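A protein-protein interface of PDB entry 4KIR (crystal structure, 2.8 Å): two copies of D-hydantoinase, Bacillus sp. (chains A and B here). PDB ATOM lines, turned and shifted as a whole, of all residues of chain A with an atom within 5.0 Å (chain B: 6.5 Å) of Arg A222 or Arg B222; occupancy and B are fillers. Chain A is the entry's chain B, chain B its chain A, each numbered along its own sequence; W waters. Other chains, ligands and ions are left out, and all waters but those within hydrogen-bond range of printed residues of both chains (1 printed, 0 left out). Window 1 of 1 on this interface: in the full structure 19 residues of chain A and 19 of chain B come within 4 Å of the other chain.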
ATOM      1  N   MET A 152      17.021   9.128   3.176  1.00  0.00           N
ATOM      2  CA  MET A 152      16.918  10.418   2.523  1.00  0.00           C
ATOM      3  C   MET A 152      15.755  10.445   1.552  1.00  0.00           C
ATOM      4  O   MET A 152      15.499  11.496   0.953  1.00  0.00           O
ATOM      5  CB  MET A 152      18.234  10.738   1.810  1.00  0.00           C
ATOM      6  CG  MET A 152      19.393  10.863   2.791  1.00  0.00           C
ATOM      7  SD  MET A 152      20.959  10.645   2.005  1.00  0.00           S
ATOM      8  CE  MET A 152      21.316  12.315   1.499  1.00  0.00           C
ATOM      9  N   ASP A 162      18.588  17.066   6.132  1.00  0.00           N
ATOM     10  CA  ASP A 162      20.059  17.166   6.295  1.00  0.00           C
ATOM     11  C   ASP A 162      20.464  17.385   7.774  1.00  0.00           C
ATOM     12  O   ASP A 162      21.458  16.846   8.242  1.00  0.00           O
ATOM     13  CB  ASP A 162      20.640  18.282   5.394  1.00  0.00           C
ATOM     14  CG  ASP A 162      20.560  17.964   3.859  1.00  0.00           C
ATOM     15  OD1 ASP A 162      20.901  16.824   3.460  1.00  0.00           O
ATOM     16  OD2 ASP A 162      20.251  18.887   3.052  1.00  0.00           O
ATOM     17  N   ASN A 185      17.297  11.384  -3.417  1.00  0.00           N
ATOM     18  CA  ASN A 185      16.636  12.617  -3.048  1.00  0.00           C
ATOM     19  C   ASN A 185      15.122  12.465  -3.103  1.00  0.00           C
ATOM     20  O   ASN A 185      14.512  12.598  -4.183  1.00  0.00           O
ATOM     21  CB  ASN A 185      17.055  13.756  -3.987  1.00  0.00           C
ATOM     22  CG  ASN A 185      16.649  15.127  -3.463  1.00  0.00           C
ATOM     23  OD1 ASN A 185      15.515  15.357  -3.020  1.00  0.00           O
ATOM     24  ND2 ASN A 185      17.591  16.035  -3.479  1.00  0.00           N
ATOM     25  N   GLY A 217      23.080   9.474  -7.291  1.00  0.00           N
ATOM     26  CA  GLY A 217      24.354  10.157  -7.365  1.00  0.00           C
ATOM     27  C   GLY A 217      24.391  11.392  -6.499  1.00  0.00           C
ATOM     28  O   GLY A 217      25.376  11.663  -5.848  1.00  0.00           O
ATOM     29  N   GLU A 218      23.284  12.107  -6.460  1.00  0.00           N
ATOM     30  CA  GLU A 218      23.207  13.338  -5.696  1.00  0.00           C
ATOM     31  C   GLU A 218      23.211  13.063  -4.186  1.00  0.00           C
ATOM     32  O   GLU A 218      24.095  13.518  -3.471  1.00  0.00           O
ATOM     33  CB  GLU A 218      21.985  14.151  -6.139  1.00  0.00           C
ATOM     34  CG  GLU A 218      21.952  15.542  -5.564  1.00  0.00           C
ATOM     35  CD  GLU A 218      21.743  15.570  -4.079  1.00  0.00           C
ATOM     36  OE1 GLU A 218      20.759  14.930  -3.631  1.00  0.00           O
ATOM     37  OE2 GLU A 218      22.589  16.194  -3.383  1.00  0.00           O
ATOM     38  N   ALA A 219      22.262  12.271  -3.721  1.00  0.00           N
ATOM     39  CA  ALA A 219      22.159  11.984  -2.278  1.00  0.00           C
ATOM     40  C   ALA A 219      23.359  11.290  -1.760  1.00  0.00           C
ATOM     41  O   ALA A 219      23.736  11.525  -0.617  1.00  0.00           O
ATOM     42  CB  ALA A 219      20.941  11.154  -1.963  1.00  0.00           C
ATOM     43  N   THR A 220      23.964  10.435  -2.593  1.00  0.00           N
ATOM     44  CA  THR A 220      25.200   9.764  -2.213  1.00  0.00           C
ATOM     45  C   THR A 220      26.291  10.822  -1.990  1.00  0.00           C
ATOM     46  O   THR A 220      26.885  10.924  -0.926  1.00  0.00           O
ATOM     47  CB  THR A 220      25.614   8.766  -3.287  1.00  0.00           C
ATOM     48  OG1 THR A 220      24.569   7.806  -3.448  1.00  0.00           O
ATOM     49  CG2 THR A 220      26.871   8.025  -2.885  1.00  0.00           C
ATOM     50  N   GLY A 221      26.457  11.683  -2.972  1.00  0.00           N
ATOM     51  CA  GLY A 221      27.414  12.734  -2.922  1.00  0.00           C
ATOM     52  C   GLY A 221      27.217  13.551  -1.689  1.00  0.00           C
ATOM     53  O   GLY A 221      28.189  13.886  -0.987  1.00  0.00           O
ATOM     54  N   ARG A 222      25.947  13.829  -1.408  1.00  0.00           N
ATOM     55  CA  ARG A 222      25.576  14.711  -0.303  1.00  0.00           C
ATOM     56  C   ARG A 222      25.933  14.083   1.012  1.00  0.00           C
ATOM     57  O   ARG A 222      26.613  14.700   1.834  1.00  0.00           O
ATOM     58  CB  ARG A 222      24.088  15.026  -0.340  1.00  0.00           C
ATOM     59  CG  ARG A 222      23.526  15.773   0.873  1.00  0.00           C
ATOM     60  CD  ARG A 222      22.373  16.662   0.416  1.00  0.00           C
ATOM     61  NE  ARG A 222      21.412  15.980  -0.480  1.00  0.00           N
ATOM     62  CZ  ARG A 222      20.246  15.443  -0.115  1.00  0.00           C
ATOM     63  NH1 ARG A 222      19.851  15.479   1.146  1.00  0.00           N
ATOM     64  NH2 ARG A 222      19.453  14.881  -1.020  1.00  0.00           N
ATOM     65  N   ALA A 223      25.519  12.840   1.188  1.00  0.00           N
ATOM     66  CA  ALA A 223      25.724  12.159   2.468  1.00  0.00           C
ATOM     67  C   ALA A 223      27.210  11.922   2.705  1.00  0.00           C
ATOM     68  O   ALA A 223      27.656  11.915   3.847  1.00  0.00           O
ATOM     69  CB  ALA A 223      24.964  10.852   2.487  1.00  0.00           C
ATOM     70  N   ILE A 224      27.988  11.809   1.619  1.00  0.00           N
ATOM     71  CA  ILE A 224      29.459  11.775   1.722  1.00  0.00           C
ATOM     72  C   ILE A 224      30.048  13.108   2.185  1.00  0.00           C
ATOM     73  O   ILE A 224      31.025  13.135   2.943  1.00  0.00           O
ATOM     74  CB  ILE A 224      30.090  11.389   0.388  1.00  0.00           C
ATOM     75  CG1 ILE A 224      29.869   9.892   0.120  1.00  0.00           C
ATOM     76  CG2 ILE A 224      31.580  11.702   0.362  1.00  0.00           C
ATOM     77  CD1 ILE A 224      29.933   9.475  -1.351  1.00  0.00           C
ATOM     78  N   ALA A 225      29.491  14.203   1.685  1.00  0.00           N
ATOM     79  CA  ALA A 225      29.999  15.504   2.015  1.00  0.00           C
ATOM     80  C   ALA A 225      29.807  15.777   3.505  1.00  0.00           C
ATOM     81  O   ALA A 225      30.773  16.154   4.189  1.00  0.00           O
ATOM     82  CB  ALA A 225      29.343  16.564   1.153  1.00  0.00           C
ATOM     83  N   LEU A 226      28.631  15.462   4.049  1.00  0.00           N
ATOM     84  CA  LEU A 226      28.413  15.646   5.511  1.00  0.00           C
ATOM     85  C   LEU A 226      29.336  14.792   6.390  1.00  0.00           C
ATOM     86  O   LEU A 226      29.909  15.263   7.381  1.00  0.00           O
ATOM     87  CB  LEU A 226      26.971  15.392   5.913  1.00  0.00           C
ATOM     88  CG  LEU A 226      25.920  16.088   5.028  1.00  0.00           C
ATOM     89  CD1 LEU A 226      24.572  16.075   5.730  1.00  0.00           C
ATOM     90  CD2 LEU A 226      26.289  17.520   4.673  1.00  0.00           C
ATOM     91  N   MET B 152      19.802  28.541  -0.624  1.00  0.00           N
ATOM     92  CA  MET B 152      19.903  27.253   0.044  1.00  0.00           C
ATOM     93  C   MET B 152      20.428  27.402   1.474  1.00  0.00           C
ATOM     94  O   MET B 152      20.457  26.422   2.219  1.00  0.00           O
ATOM     95  CB  MET B 152      20.784  26.307  -0.778  1.00  0.00           C
ATOM     96  CG  MET B 152      20.222  26.025  -2.151  1.00  0.00           C
ATOM     97  SD  MET B 152      21.484  25.457  -3.286  1.00  0.00           S
ATOM     98  CE  MET B 152      21.390  23.723  -2.978  1.00  0.00           C
ATOM     99  N   ALA B 160      15.313  27.775   1.212  1.00  0.00           N
ATOM    100  CA  ALA B 160      14.311  26.972   0.489  1.00  0.00           C
ATOM    101  C   ALA B 160      14.682  25.504   0.439  1.00  0.00           C
ATOM    102  O   ALA B 160      15.841  25.168   0.301  1.00  0.00           O
ATOM    103  CB  ALA B 160      14.158  27.483  -0.933  1.00  0.00           C
ATOM    104  N   ASP B 161      13.698  24.624   0.521  1.00  0.00           N
ATOM    105  CA  ASP B 161      13.964  23.176   0.404  1.00  0.00           C
ATOM    106  C   ASP B 161      14.101  22.700  -1.056  1.00  0.00           C
ATOM    107  O   ASP B 161      13.809  23.479  -2.020  1.00  0.00           O
ATOM    108  CB  ASP B 161      12.981  22.323   1.199  1.00  0.00           C
ATOM    109  CG  ASP B 161      11.555  22.543   0.812  1.00  0.00           C
ATOM    110  OD1 ASP B 161      10.695  22.361   1.700  1.00  0.00           O
ATOM    111  OD2 ASP B 161      11.275  22.898  -0.348  1.00  0.00           O
ATOM    112  N   ASP B 162      14.648  21.481  -1.193  1.00  0.00           N
ATOM    113  CA  ASP B 162      14.962  20.930  -2.493  1.00  0.00           C
ATOM    114  C   ASP B 162      13.702  20.943  -3.361  1.00  0.00           C
ATOM    115  O   ASP B 162      13.765  21.301  -4.536  1.00  0.00           O
ATOM    116  CB  ASP B 162      15.561  19.537  -2.390  1.00  0.00           C
ATOM    117  CG  ASP B 162      17.010  19.529  -1.820  1.00  0.00           C
ATOM    118  OD1 ASP B 162      17.892  20.272  -2.299  1.00  0.00           O
ATOM    119  OD2 ASP B 162      17.299  18.718  -0.914  1.00  0.00           O
ATOM    120  N   LEU B 165      13.358  24.413  -4.740  1.00  0.00           N
ATOM    121  CA  LEU B 165      14.479  24.435  -5.696  1.00  0.00           C
ATOM    122  C   LEU B 165      14.152  23.708  -7.022  1.00  0.00           C
ATOM    123  O   LEU B 165      14.194  24.323  -8.104  1.00  0.00           O
ATOM    124  CB  LEU B 165      15.765  23.871  -5.064  1.00  0.00           C
ATOM    125  CG  LEU B 165      17.117  24.552  -5.349  1.00  0.00           C
ATOM    126  CD1 LEU B 165      18.315  23.630  -5.064  1.00  0.00           C
ATOM    127  CD2 LEU B 165      17.268  25.106  -6.749  1.00  0.00           C
ATOM    128  N   GLU B 184      24.970  27.202  -0.294  1.00  0.00           N
ATOM    129  CA  GLU B 184      25.573  26.618   0.928  1.00  0.00           C
ATOM    130  C   GLU B 184      24.500  25.873   1.658  1.00  0.00           C
ATOM    131  O   GLU B 184      23.368  26.301   1.684  1.00  0.00           O
ATOM    132  CB  GLU B 184      26.140  27.672   1.874  1.00  0.00           C
ATOM    133  CG  GLU B 184      27.240  28.537   1.293  1.00  0.00           C
ATOM    134  CD  GLU B 184      28.040  29.260   2.356  1.00  0.00           C
ATOM    135  OE1 GLU B 184      27.624  30.395   2.701  1.00  0.00           O
ATOM    136  OE2 GLU B 184      29.093  28.681   2.774  1.00  0.00           O
ATOM    137  N   ASN B 185      24.878  24.795   2.310  1.00  0.00           N
ATOM    138  CA  ASN B 185      23.930  23.991   3.046  1.00  0.00           C
ATOM    139  C   ASN B 185      23.602  24.661   4.379  1.00  0.00           C
ATOM    140  O   ASN B 185      24.269  24.406   5.392  1.00  0.00           O
ATOM    141  CB  ASN B 185      24.498  22.587   3.293  1.00  0.00           C
ATOM    142  CG  ASN B 185      23.453  21.621   3.777  1.00  0.00           C
ATOM    143  OD1 ASN B 185      22.686  21.913   4.688  1.00  0.00           O
ATOM    144  ND2 ASN B 185      23.396  20.471   3.163  1.00  0.00           N
ATOM    145  N   GLY B 186      22.527  25.453   4.378  1.00  0.00           N
ATOM    146  CA  GLY B 186      21.919  25.973   5.614  1.00  0.00           C
ATOM    147  C   GLY B 186      21.982  25.033   6.816  1.00  0.00           C
ATOM    148  O   GLY B 186      22.609  25.349   7.826  1.00  0.00           O
ATOM    149  N   ASP B 187      21.451  23.827   6.652  1.00  0.00           N
ATOM    150  CA  ASP B 187      21.334  22.881   7.768  1.00  0.00           C
ATOM    151  C   ASP B 187      22.671  22.615   8.449  1.00  0.00           C
ATOM    152  O   ASP B 187      22.755  22.746   9.656  1.00  0.00           O
ATOM    153  CB  ASP B 187      20.659  21.570   7.342  1.00  0.00           C
ATOM    154  CG  ASP B 187      19.275  21.789   6.722  1.00  0.00           C
ATOM    155  OD1 ASP B 187      18.389  22.324   7.406  1.00  0.00           O
ATOM    156  OD2 ASP B 187      19.077  21.481   5.525  1.00  0.00           O
ATOM    157  N   ALA B 215      30.769  22.698   2.455  1.00  0.00           N
ATOM    158  CA  ALA B 215      29.334  23.008   2.447  1.00  0.00           C
ATOM    159  C   ALA B 215      28.841  23.811   1.232  1.00  0.00           C
ATOM    160  O   ALA B 215      27.630  23.870   0.991  1.00  0.00           O
ATOM    161  CB  ALA B 215      28.985  23.781   3.707  1.00  0.00           C
ATOM    162  N   GLY B 217      30.639  23.443  -1.791  1.00  0.00           N
ATOM    163  CA  GLY B 217      30.845  22.380  -2.744  1.00  0.00           C
ATOM    164  C   GLY B 217      29.611  21.511  -2.813  1.00  0.00           C
ATOM    165  O   GLY B 217      29.192  21.083  -3.895  1.00  0.00           O
ATOM    166  N   GLU B 218      29.035  21.243  -1.644  1.00  0.00           N
ATOM    167  CA  GLU B 218      27.946  20.300  -1.559  1.00  0.00           C
ATOM    168  C   GLU B 218      26.703  20.901  -2.199  1.00  0.00           C
ATOM    169  O   GLU B 218      26.114  20.305  -3.097  1.00  0.00           O
ATOM    170  CB  GLU B 218      27.731  19.881  -0.105  1.00  0.00           C
ATOM    171  CG  GLU B 218      26.694  18.807   0.051  1.00  0.00           C
ATOM    172  CD  GLU B 218      25.300  19.316  -0.310  1.00  0.00           C
ATOM    173  OE1 GLU B 218      24.853  20.316   0.316  1.00  0.00           O
ATOM    174  OE2 GLU B 218      24.680  18.748  -1.266  1.00  0.00           O
ATOM    175  N   ALA B 219      26.309  22.083  -1.751  1.00  0.00           N
ATOM    176  CA  ALA B 219      25.097  22.702  -2.289  1.00  0.00           C
ATOM    177  C   ALA B 219      25.216  23.031  -3.760  1.00  0.00           C
ATOM    178  O   ALA B 219      24.236  22.933  -4.514  1.00  0.00           O
ATOM    179  CB  ALA B 219      24.727  23.946  -1.512  1.00  0.00           C
ATOM    180  N   THR B 220      26.399  23.451  -4.176  1.00  0.00           N
ATOM    181  CA  THR B 220      26.636  23.754  -5.616  1.00  0.00           C
ATOM    182  C   THR B 220      26.402  22.508  -6.429  1.00  0.00           C
ATOM    183  O   THR B 220      25.581  22.527  -7.323  1.00  0.00           O
ATOM    184  CB  THR B 220      28.071  24.217  -5.844  1.00  0.00           C
ATOM    185  OG1 THR B 220      28.279  25.424  -5.109  1.00  0.00           O
ATOM    186  CG2 THR B 220      28.318  24.502  -7.264  1.00  0.00           C
ATOM    187  N   GLY B 221      27.034  21.407  -5.992  1.00  0.00           N
ATOM    188  CA  GLY B 221      26.856  20.086  -6.569  1.00  0.00           C
ATOM    189  C   GLY B 221      25.404  19.674  -6.643  1.00  0.00           C
ATOM    190  O   GLY B 221      24.935  19.195  -7.665  1.00  0.00           O
ATOM    191  N   ARG B 222      24.694  19.907  -5.550  1.00  0.00           N
ATOM    192  CA  ARG B 222      23.314  19.517  -5.426  1.00  0.00           C
ATOM    193  C   ARG B 222      22.509  20.274  -6.386  1.00  0.00           C
ATOM    194  O   ARG B 222      21.693  19.694  -7.086  1.00  0.00           O
ATOM    195  CB  ARG B 222      22.819  19.802  -4.024  1.00  0.00           C
ATOM    196  CG  ARG B 222      21.327  19.624  -3.817  1.00  0.00           C
ATOM    197  CD  ARG B 222      21.052  19.122  -2.405  1.00  0.00           C
ATOM    198  NE  ARG B 222      21.812  19.847  -1.374  1.00  0.00           N
ATOM    199  CZ  ARG B 222      21.361  20.883  -0.678  1.00  0.00           C
ATOM    200  NH1 ARG B 222      20.111  21.351  -0.850  1.00  0.00           N
ATOM    201  NH2 ARG B 222      22.155  21.449   0.226  1.00  0.00           N
ATOM    202  N   ALA B 223      22.731  21.580  -6.433  1.00  0.00           N
ATOM    203  CA  ALA B 223      21.897  22.439  -7.291  1.00  0.00           C
ATOM    204  C   ALA B 223      22.157  22.141  -8.772  1.00  0.00           C
ATOM    205  O   ALA B 223      21.251  22.213  -9.615  1.00  0.00           O
ATOM    206  CB  ALA B 223      22.128  23.911  -6.979  1.00  0.00           C
ATOM    207  N   ILE B 224      23.384  21.729  -9.069  1.00  0.00           N
ATOM    208  CA  ILE B 224      23.719  21.288 -10.414  1.00  0.00           C
ATOM    209  C   ILE B 224      22.925  20.015 -10.772  1.00  0.00           C
ATOM    210  O   ILE B 224      22.416  19.870 -11.894  1.00  0.00           O
ATOM    211  CB  ILE B 224      25.241  21.075 -10.526  1.00  0.00           C
ATOM    212  CG1 ILE B 224      25.949  22.447 -10.629  1.00  0.00           C
ATOM    213  CG2 ILE B 224      25.605  20.221 -11.714  1.00  0.00           C
ATOM    214  CD1 ILE B 224      27.430  22.437 -10.263  1.00  0.00           C
ATOM    215  N   ALA B 225      22.835  19.097  -9.814  1.00  0.00           N
ATOM    216  CA  ALA B 225      22.224  17.831 -10.062  1.00  0.00           C
ATOM    217  C   ALA B 225      20.774  18.035 -10.401  1.00  0.00           C
ATOM    218  O   ALA B 225      20.326  17.513 -11.431  1.00  0.00           O
ATOM    219  CB  ALA B 225      22.384  16.920  -8.882  1.00  0.00           C
ATOM    220  N   LEU B 226      20.062  18.878  -9.651  1.00  0.00           N
ATOM    221  CA  LEU B 226      18.622  19.111  -9.986  1.00  0.00           C
ATOM    222  C   LEU B 226      18.420  19.760 -11.357  1.00  0.00           C
ATOM    223  O   LEU B 226      17.527  19.375 -12.107  1.00  0.00           O
ATOM    224  CB  LEU B 226      17.917  19.929  -8.926  1.00  0.00           C
ATOM    225  CG  LEU B 226      18.164  19.488  -7.492  1.00  0.00           C
ATOM    226  CD1 LEU B 226      17.183  20.186  -6.576  1.00  0.00           C
ATOM    227  CD2 LEU B 226      18.053  18.003  -7.308  1.00  0.00           C
ATOM    228  N   THR B 227      19.282  20.730 -11.672  1.00  0.00           N
ATOM    229  CA  THR B 227      19.324  21.386 -12.987  1.00  0.00           C
ATOM    230  C   THR B 227      19.443  20.337 -14.123  1.00  0.00           C
ATOM    231  O   THR B 227      18.675  20.336 -15.039  1.00  0.00           O
ATOM    232  CB  THR B 227      20.497  22.414 -13.011  1.00  0.00           C
ATOM    233  OG1 THR B 227      20.367  23.293 -11.900  1.00  0.00           O
ATOM    234  CG2 THR B 227      20.551  23.254 -14.310  1.00  0.00           C
ATOM    235  N   LEU B 234      21.366  26.985 -14.853  1.00  0.00           N
ATOM    236  CA  LEU B 234      21.745  27.429 -13.494  1.00  0.00           C
ATOM    237  C   LEU B 234      22.826  28.451 -13.529  1.00  0.00           C
ATOM    238  O   LEU B 234      23.648  28.409 -14.400  1.00  0.00           O
ATOM    239  CB  LEU B 234      22.220  26.245 -12.621  1.00  0.00           C
ATOM    240  CG  LEU B 234      22.383  26.523 -11.104  1.00  0.00           C
ATOM    241  CD1 LEU B 234      21.040  26.873 -10.442  1.00  0.00           C
ATOM    242  CD2 LEU B 234      23.045  25.364 -10.355  1.00  0.00           C
ATOM    243  N   ARG B 247      32.865  21.446  -9.187  1.00  0.00           N
ATOM    244  CA  ARG B 247      31.523  20.922  -9.463  1.00  0.00           C
ATOM    245  C   ARG B 247      30.899  21.544 -10.707  1.00  0.00           C
ATOM    246  O   ARG B 247      30.210  20.840 -11.470  1.00  0.00           O
ATOM    247  CB  ARG B 247      30.604  21.152  -8.256  1.00  0.00           C
ATOM    248  CG  ARG B 247      30.356  19.965  -7.325  1.00  0.00           C
ATOM    249  CD  ARG B 247      31.600  19.224  -6.887  1.00  0.00           C
ATOM    250  NE  ARG B 247      31.304  17.864  -6.407  1.00  0.00           N
ATOM    251  CZ  ARG B 247      32.169  16.840  -6.408  1.00  0.00           C
ATOM    252  NH1 ARG B 247      33.429  16.982  -6.839  1.00  0.00           N
ATOM    253  NH2 ARG B 247      31.764  15.637  -5.998  1.00  0.00           N
HETATM  254  O   HOH W   1      18.660  18.475   1.185  1.00  0.00           O
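Of the 23 printed residues of chain B, 6 touch a printed residue of chain A.
Printed residues of chain B that touch a printed residue of chain A: Asp B162, Asn B185, Asp B187, Glu B218, Arg B222 and Ala B225.
Hydrophobic or aromatic side chains of chain B that line the printed part of chain A: Ala B225.
Along chain B the printed residues that touch a printed residue of chain A span positions 162 to 225.
Along chain A the printed residues that touch a printed residue of chain B span positions 162 to 225.
OD2 of Asp A162 touches ND2 of Asn B185, 3.5 Å away.
Asp B187 touches Asp A162 (OD2 to CB, 3.6 Å).
Asn A185 touches Asp B162 (ND2 to OD2, 3.7 Å).
Glu A218 touches Glu B218 (OE2 to OE2, 3.9 Å).
Glu A218 touches Arg B222 (OE2 to CD, 3.4 Å).
Glu A218 touches Ala B225.
Arg A222 touches Glu B218.
Arg A222 touches Arg B222.
CG of Glu B218 touches CB of Ala A225 (3.6 Å).
Asp A162 touches Asn B185, and with the chains exchanged Asn A185 touches Asp B162.
Glu A218 touches Arg B222, and with the chains exchanged Arg A222 touches Glu B218.
Glu A218 touches Ala B225, and with the chains exchanged Ala A225 touches Glu B218.
Arg A222 touches its own counterpart, Arg B222.
Water W1 lies within hydrogen-bond range of OD2 of Asp A162 (2.5 Å), OD2 of Asp B162 (2.5 Å) and NH1 of Arg A222 (3.2 Å).
The guanidinium group of Arg A222 is in salt-bridge range of the side-chain carboxylate of Glu A218 (2.9 Å).
The side-chain carboxylate (OD1) of Asp A162 lies within salt-bridge range of the guanidinium group (NH1) of Arg A222 (2.9 Å).
The backbone NH (N) of Asn B185 lies within hydrogen-bond range of the backbone carbonyl oxygen (O) of Ala B215, 3.2 Å away.
The side-chain amide nitrogen of Asn A185 sits close to the guanidinium group of Arg A222.
The guanidinium group of Arg B222 is in salt-bridge range of the side-chain carboxylate of Asp B162 (2.9 Å).
The side-chain amide oxygen (OD1) of Asn B185 sits at hydrogen-bond distance from the backbone NH (N) of Asp B187, at 3.0 Å.
Of the printed residues of chain B, Asp A162 touches Asn B185 and Asp B187.
Of the printed residues of chain B, Asn A185 touches Asp B162 (3.7 Å).
Of the printed residues of chain B, Glu A218 touches Glu B218 (3.9 Å), Arg B222 (3.4 Å) and Ala B225 (3.6 Å).
Arg A222 touches just these residues of chain B: Glu B218 and Arg B222.
Leu A226 touches none of the printed residues of chain B.
Of the printed residues of chain A, Asp B162 touches Asn A185 (3.7 Å).
Of the printed residues of chain A, Asn B185 touches Asp A162 (3.5 Å).
Of chain A, only Glu A218 (3.4 Å) and Arg A222 (3.7 Å) come within 4 Å of Arg B222.
Ala B223 touches none of the printed residues of chain A.
The nearest residue of chain B that does not touch Arg A222 is Asp B162 (4.4 Å).
The nearest residue of chain A that does not touch Arg B222 is Asp A162 (4.3 Å).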
